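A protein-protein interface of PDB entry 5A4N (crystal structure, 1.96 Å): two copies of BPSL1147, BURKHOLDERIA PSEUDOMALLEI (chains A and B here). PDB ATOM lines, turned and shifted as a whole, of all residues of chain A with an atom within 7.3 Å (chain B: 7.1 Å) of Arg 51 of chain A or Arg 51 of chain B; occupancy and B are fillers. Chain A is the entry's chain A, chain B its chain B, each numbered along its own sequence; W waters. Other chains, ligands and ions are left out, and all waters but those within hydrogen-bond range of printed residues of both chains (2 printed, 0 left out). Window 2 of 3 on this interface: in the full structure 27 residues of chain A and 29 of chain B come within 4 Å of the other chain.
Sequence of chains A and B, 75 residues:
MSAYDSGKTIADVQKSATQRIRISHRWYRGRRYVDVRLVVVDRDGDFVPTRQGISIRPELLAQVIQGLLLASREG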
ATOM      1  N   ARG A  37       2.709  -7.066  -4.027  1.00  0.00           N
ATOM      2  CA  ARG A  37       2.667  -6.075  -2.958  1.00  0.00           C
ATOM      3  C   ARG A  37       1.809  -6.493  -1.780  1.00  0.00           C
ATOM      4  O   ARG A  37       0.742  -7.081  -1.940  1.00  0.00           O
ATOM      5  CB  ARG A  37       2.149  -4.756  -3.539  1.00  0.00           C
ATOM      6  CG  ARG A  37       2.342  -3.506  -2.678  1.00  0.00           C
ATOM      7  CD  ARG A  37       2.036  -2.250  -3.495  1.00  0.00           C
ATOM      8  NE  ARG A  37       2.995  -2.198  -4.582  1.00  0.00           N
ATOM      9  CZ  ARG A  37       4.226  -1.706  -4.500  1.00  0.00           C
ATOM     10  NH1 ARG A  37       4.664  -1.101  -3.409  1.00  0.00           N
ATOM     11  NH2 ARG A  37       5.008  -1.761  -5.548  1.00  0.00           N
ATOM     12  N   LEU A  38       2.288  -6.176  -0.583  1.00  0.00           N
ATOM     13  CA  LEU A  38       1.471  -6.263   0.626  1.00  0.00           C
ATOM     14  C   LEU A  38       0.393  -5.157   0.678  1.00  0.00           C
ATOM     15  O   LEU A  38       0.693  -3.955   0.563  1.00  0.00           O
ATOM     16  CB  LEU A  38       2.381  -6.196   1.841  1.00  0.00           C
ATOM     17  CG  LEU A  38       1.743  -6.322   3.223  1.00  0.00           C
ATOM     18  CD1 LEU A  38       1.213  -7.731   3.438  1.00  0.00           C
ATOM     19  CD2 LEU A  38       2.781  -5.952   4.274  1.00  0.00           C
ATOM     20  N   VAL A  48      -5.394  -1.219   1.445  1.00  0.00           N
ATOM     21  CA  VAL A  48      -4.645  -0.188   0.759  1.00  0.00           C
ATOM     22  C   VAL A  48      -3.254  -0.720   0.519  1.00  0.00           C
ATOM     23  O   VAL A  48      -2.686  -1.345   1.398  1.00  0.00           O
ATOM     24  CB  VAL A  48      -4.571   1.155   1.554  1.00  0.00           C
ATOM     25  CG1 VAL A  48      -5.961   1.649   1.911  1.00  0.00           C
ATOM     26  CG2 VAL A  48      -3.736   1.027   2.825  1.00  0.00           C
ATOM     27  N   PRO A  49      -2.683  -0.437  -0.661  1.00  0.00           N
ATOM     28  CA  PRO A  49      -1.320  -0.867  -0.902  1.00  0.00           C
ATOM     29  C   PRO A  49      -0.341  -0.196   0.056  1.00  0.00           C
ATOM     30  O   PRO A  49      -0.596   0.912   0.520  1.00  0.00           O
ATOM     31  CB  PRO A  49      -1.066  -0.435  -2.351  1.00  0.00           C
ATOM     32  CG  PRO A  49      -1.943   0.746  -2.535  1.00  0.00           C
ATOM     33  CD  PRO A  49      -3.179   0.448  -1.728  1.00  0.00           C
ATOM     34  N   THR A  50       0.712  -0.924   0.403  1.00  0.00           N
ATOM     35  CA  THR A  50       1.823  -0.431   1.189  1.00  0.00           C
ATOM     36  C   THR A  50       3.035  -0.274   0.293  1.00  0.00           C
ATOM     37  O   THR A  50       2.976  -0.649  -0.865  1.00  0.00           O
ATOM     38  CB  THR A  50       2.191  -1.407   2.316  1.00  0.00           C
ATOM     39  OG1 THR A  50       2.691  -2.631   1.761  1.00  0.00           O
ATOM     40  CG2 THR A  50       0.982  -1.677   3.175  1.00  0.00           C
ATOM     41  N   ARG A  51       4.129   0.260   0.840  1.00  0.00           N
ATOM     42  CA  ARG A  51       5.438   0.329   0.159  1.00  0.00           C
ATOM     43  C   ARG A  51       6.188  -0.982   0.166  1.00  0.00           C
ATOM     44  O   ARG A  51       7.290  -1.009  -0.359  1.00  0.00           O
ATOM     45  CB  ARG A  51       6.399   1.308   0.864  1.00  0.00           C
ATOM     46  CG  ARG A  51       6.121   2.799   0.699  1.00  0.00           C
ATOM     47  CD  ARG A  51       7.325   3.603   1.228  1.00  0.00           C
ATOM     48  NE  ARG A  51       7.127   5.048   1.212  1.00  0.00           N
ATOM     49  CZ  ARG A  51       7.197   5.829   0.128  1.00  0.00           C
ATOM     50  NH1 ARG A  51       7.461   5.321  -1.076  1.00  0.00           N
ATOM     51  NH2 ARG A  51       6.999   7.138   0.253  1.00  0.00           N
ATOM     52  N   GLN A  52       5.664  -2.027   0.822  1.00  0.00           N
ATOM     53  CA  GLN A  52       6.322  -3.307   0.863  1.00  0.00           C
ATOM     54  C   GLN A  52       5.895  -4.081  -0.361  1.00  0.00           C
ATOM     55  O   GLN A  52       4.904  -4.820  -0.347  1.00  0.00           O
ATOM     56  CB  GLN A  52       5.966  -4.038   2.130  1.00  0.00           C
ATOM     57  CG  GLN A  52       6.421  -3.211   3.325  1.00  0.00           C
ATOM     58  CD  GLN A  52       6.086  -3.857   4.632  1.00  0.00           C
ATOM     59  OE1 GLN A  52       5.647  -3.186   5.566  1.00  0.00           O
ATOM     60  NE2 GLN A  52       6.298  -5.160   4.717  1.00  0.00           N
ATOM     61  N   GLY A  53       6.644  -3.886  -1.434  1.00  0.00           N
ATOM     62  CA  GLY A  53       6.290  -4.500  -2.695  1.00  0.00           C
ATOM     63  C   GLY A  53       7.404  -4.350  -3.680  1.00  0.00           C
ATOM     64  O   GLY A  53       8.354  -3.590  -3.463  1.00  0.00           O
ATOM     65  N   ILE A  54       7.278  -5.091  -4.768  1.00  0.00           N
ATOM     66  CA  ILE A  54       8.331  -5.180  -5.744  1.00  0.00           C
ATOM     67  C   ILE A  54       7.745  -5.214  -7.165  1.00  0.00           C
ATOM     68  O   ILE A  54       6.622  -5.695  -7.361  1.00  0.00           O
ATOM     69  CB  ILE A  54       9.240  -6.369  -5.406  1.00  0.00           C
ATOM     70  CG1 ILE A  54      10.505  -6.326  -6.247  1.00  0.00           C
ATOM     71  CG2 ILE A  54       8.529  -7.703  -5.640  1.00  0.00           C
ATOM     72  CD1 ILE A  54      11.627  -7.202  -5.695  1.00  0.00           C
ATOM     73  N   ARG B  37      12.643 -10.016  -2.287  1.00  0.00           N
ATOM     74  CA  ARG B  37      13.057  -8.664  -1.850  1.00  0.00           C
ATOM     75  C   ARG B  37      14.049  -8.021  -2.811  1.00  0.00           C
ATOM     76  O   ARG B  37      14.945  -8.687  -3.328  1.00  0.00           O
ATOM     77  CB  ARG B  37      13.711  -8.767  -0.499  1.00  0.00           C
ATOM     78  CG  ARG B  37      13.885  -7.458   0.268  1.00  0.00           C
ATOM     79  CD  ARG B  37      14.098  -7.704   1.764  1.00  0.00           C
ATOM     80  NE  ARG B  37      12.921  -8.351   2.289  1.00  0.00           N
ATOM     81  CZ  ARG B  37      11.803  -7.709   2.618  1.00  0.00           C
ATOM     82  NH1 ARG B  37      11.721  -6.358   2.573  1.00  0.00           N
ATOM     83  NH2 ARG B  37      10.763  -8.404   3.030  1.00  0.00           N
ATOM     84  N   LEU B  38      13.871  -6.738  -3.076  1.00  0.00           N
ATOM     85  CA  LEU B  38      14.877  -6.019  -3.837  1.00  0.00           C
ATOM     86  C   LEU B  38      16.075  -5.818  -2.916  1.00  0.00           C
ATOM     87  O   LEU B  38      15.942  -5.299  -1.789  1.00  0.00           O
ATOM     88  CB  LEU B  38      14.334  -4.685  -4.299  1.00  0.00           C
ATOM     89  CG  LEU B  38      15.299  -3.769  -5.055  1.00  0.00           C
ATOM     90  CD1 LEU B  38      15.640  -4.333  -6.422  1.00  0.00           C
ATOM     91  CD2 LEU B  38      14.699  -2.363  -5.173  1.00  0.00           C
ATOM     92  N   PRO B  49      19.242  -5.064   1.912  1.00  0.00           N
ATOM     93  CA  PRO B  49      17.849  -5.297   1.596  1.00  0.00           C
ATOM     94  C   PRO B  49      17.059  -4.039   1.858  1.00  0.00           C
ATOM     95  O   PRO B  49      17.317  -3.274   2.816  1.00  0.00           O
ATOM     96  CB  PRO B  49      17.452  -6.390   2.591  1.00  0.00           C
ATOM     97  CG  PRO B  49      18.279  -6.075   3.826  1.00  0.00           C
ATOM     98  CD  PRO B  49      19.580  -5.547   3.275  1.00  0.00           C
ATOM     99  N   THR B  50      16.125  -3.785   0.988  1.00  0.00           N
ATOM    100  CA  THR B  50      15.318  -2.625   1.123  1.00  0.00           C
ATOM    101  C   THR B  50      14.024  -3.125   1.711  1.00  0.00           C
ATOM    102  O   THR B  50      13.820  -4.343   1.845  1.00  0.00           O
ATOM    103  CB  THR B  50      15.113  -2.013  -0.253  1.00  0.00           C
ATOM    104  OG1 THR B  50      14.349  -2.919  -1.053  1.00  0.00           O
ATOM    105  CG2 THR B  50      16.464  -1.797  -0.891  1.00  0.00           C
ATOM    106  N   ARG B  51      13.126  -2.208   2.005  1.00  0.00           N
ATOM    107  CA  ARG B  51      11.788  -2.566   2.405  1.00  0.00           C
ATOM    108  C   ARG B  51      10.918  -3.029   1.226  1.00  0.00           C
ATOM    109  O   ARG B  51       9.769  -3.357   1.412  1.00  0.00           O
ATOM    110  CB  ARG B  51      11.168  -1.370   3.134  1.00  0.00           C
ATOM    111  CG  ARG B  51      10.657  -0.247   2.231  1.00  0.00           C
ATOM    112  CD  ARG B  51       9.849   0.738   3.045  1.00  0.00           C
ATOM    113  NE  ARG B  51      10.737   1.740   3.584  1.00  0.00           N
ATOM    114  CZ  ARG B  51      11.112   2.822   2.916  1.00  0.00           C
ATOM    115  NH1 ARG B  51      10.649   3.040   1.686  1.00  0.00           N
ATOM    116  NH2 ARG B  51      11.936   3.697   3.483  1.00  0.00           N
ATOM    117  N   GLN B  52      11.471  -2.999   0.008  1.00  0.00           N
ATOM    118  CA  GLN B  52      10.765  -3.357  -1.221  1.00  0.00           C
ATOM    119  C   GLN B  52      10.751  -4.904  -1.364  1.00  0.00           C
ATOM    120  O   GLN B  52      11.543  -5.474  -2.084  1.00  0.00           O
ATOM    121  CB  GLN B  52      11.485  -2.761  -2.448  1.00  0.00           C
ATOM    122  CG  GLN B  52      11.078  -1.365  -2.945  1.00  0.00           C
ATOM    123  CD  GLN B  52      11.091  -0.275  -1.886  1.00  0.00           C
ATOM    124  OE1 GLN B  52      12.153   0.224  -1.469  1.00  0.00           O
ATOM    125  NE2 GLN B  52       9.865   0.149  -1.479  1.00  0.00           N
ATOM    126  N   GLY B  53       9.839  -5.562  -0.681  1.00  0.00           N
ATOM    127  CA  GLY B  53       9.826  -7.033  -0.672  1.00  0.00           C
ATOM    128  C   GLY B  53       8.665  -7.571   0.123  1.00  0.00           C
ATOM    129  O   GLY B  53       7.967  -6.830   0.794  1.00  0.00           O
ATOM    130  N   ILE B  54       8.440  -8.879   0.023  1.00  0.00           N
ATOM    131  CA  ILE B  54       7.307  -9.521   0.672  1.00  0.00           C
ATOM    132  C   ILE B  54       7.774 -10.845   1.317  1.00  0.00           C
ATOM    133  O   ILE B  54       8.715 -11.457   0.868  1.00  0.00           O
ATOM    134  CB  ILE B  54       6.176  -9.802  -0.314  1.00  0.00           C
ATOM    135  CG1 ILE B  54       6.728 -10.512  -1.545  1.00  0.00           C
ATOM    136  CG2 ILE B  54       5.453  -8.527  -0.755  1.00  0.00           C
ATOM    137  CD1 ILE B  54       6.229 -11.910  -1.626  1.00  0.00           C
HETATM  138  O   HOH W   1       9.272  -4.894   3.551  1.00  0.00           O
HETATM  139  O   HOH W   2       7.878  -7.319   3.600  1.00  0.00           O
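The side-chain amide nitrogen (NE2) of Gln 52 of chain B lies within hydrogen-bond range of the backbone carbonyl oxygen (O) of Arg 51 of chain A, at 3.0 Å.
The backbone NH (N) of Leu 38 of chain A sits at hydrogen-bond distance from the backbone carbonyl oxygen (O) of Gln 52 of chain A (3.0 Å). N of Gln 52 of chain A lies within hydrogen-bond range of OG1 of Thr 50 of chain A, 3.2 Å away. NH1 of Arg 37 of chain B sits at hydrogen-bond distance from O of Thr 50 of chain B, 3.0 Å away. The backbone carbonyl oxygen (O) of Leu 38 of chain B sits at hydrogen-bond distance from the side-chain hydroxyl (OG1) of Thr 50 of chain B (3.0 Å). N of Leu 38 of chain B is in hydrogen-bond range of O of Gln 52 of chain B, 2.8 Å away. N of Gln 52 of chain B is in hydrogen-bond range of OG1 of Thr 50 of chain B, at 3.1 Å.
Among the printed residues, merely in contact across the chains: Leu 38 of chain A with Ile 54 of chain B, Arg 51 of chain A with Arg 51 of chain B, Gln 52 of chain A with Arg 51 of chain B, Gln 52 of chain A with Gly 53 of chain B, Gln 52 of chain A with Ile 54 of chain B, Gly 53 of chain A with Gln 52 of chain B, Gly 53 of chain A with Gly 53 of chain B, Ile 54 of chain A with Arg 37 of chain B and Ile 54 of chain A with Leu 38 of chain B.
Val 48 of chain A touches none of the printed residues of chain B. Arg 51 of chain A touches just these residues of chain B: Arg 51 (3.4 Å) and Gln 52 (3.0 Å). Printed residues of chain B within 4 Å of Gln 52 of chain A: Arg 51, Gly 53 and Ile 54. Printed residues of chain A within 4 Å of Leu 38 of chain B: Ile 54. Thr 50 of chain B touches none of the printed residues of chain A. Arg 51 of chain B touches just these residues of chain A: Arg 51 (3.4 Å) and Gln 52 (3.5 Å). Of the printed residues of chain A, Gln 52 of chain B touches Arg 51 (3.0 Å) and Gly 53 (3.3 Å). Of the printed residues of chain A, Gly 53 of chain B touches Gln 52 (3.6 Å) and Gly 53 (3.7 Å). The nearest printed residue of chain A that does not touch Arg 37 of chain B is Gln 52 of chain A (5.8 Å).
Of the 8 printed residues of chain B, 6 touch a printed residue of chain A. Hydrophobic or aromatic side chains of chain B within 4 Å of the printed part of chain A: Leu 38 and Ile 54. Of the 9 printed residues of chain A, 5 touch a printed residue of chain B. Hydrophobic or aromatic side chains of chain A that line the printed part of chain B: Ile 54. Among the printed residues, no Asp or Glu carboxylate lies within 4 Å of a Lys or Arg side-chain nitrogen of the other chain.
Arg 51 of chain A touches its own counterpart, Arg 51 of chain B. Arg 51 of chain A touches Gln 52 of chain B, and with the chains exchanged Gln 52 of chain A touches Arg 51 of chain B. Gly 53 of chain B touches its own counterpart, Gly 53 of chain A. Ile 54 of chain A touches Arg 37 of chain B, but with the chains exchanged Arg 37 of chain A does not touch Ile 54 of chain B (4.3 Å). Of the 10 pairs that touch across the chains among the printed residues, 8 have their exchanged pair printed and touching as well.
Water W1 lies within hydrogen-bond range of the backbone carbonyl oxygen (O) of Arg 51 of chain B (2.7 Å), the guanidinium group (NH1) of Arg 37 of chain B (3.0 Å) and the side-chain amide nitrogen (NE2) of Gln 52 of chain A (3.2 Å). Water W2 lies within hydrogen-bond range of O of Gly 53 of chain B (2.8 Å), NE2 of Gln 52 of chain A (2.9 Å) and NH2 of Arg 37 of chain B (3.1 Å).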
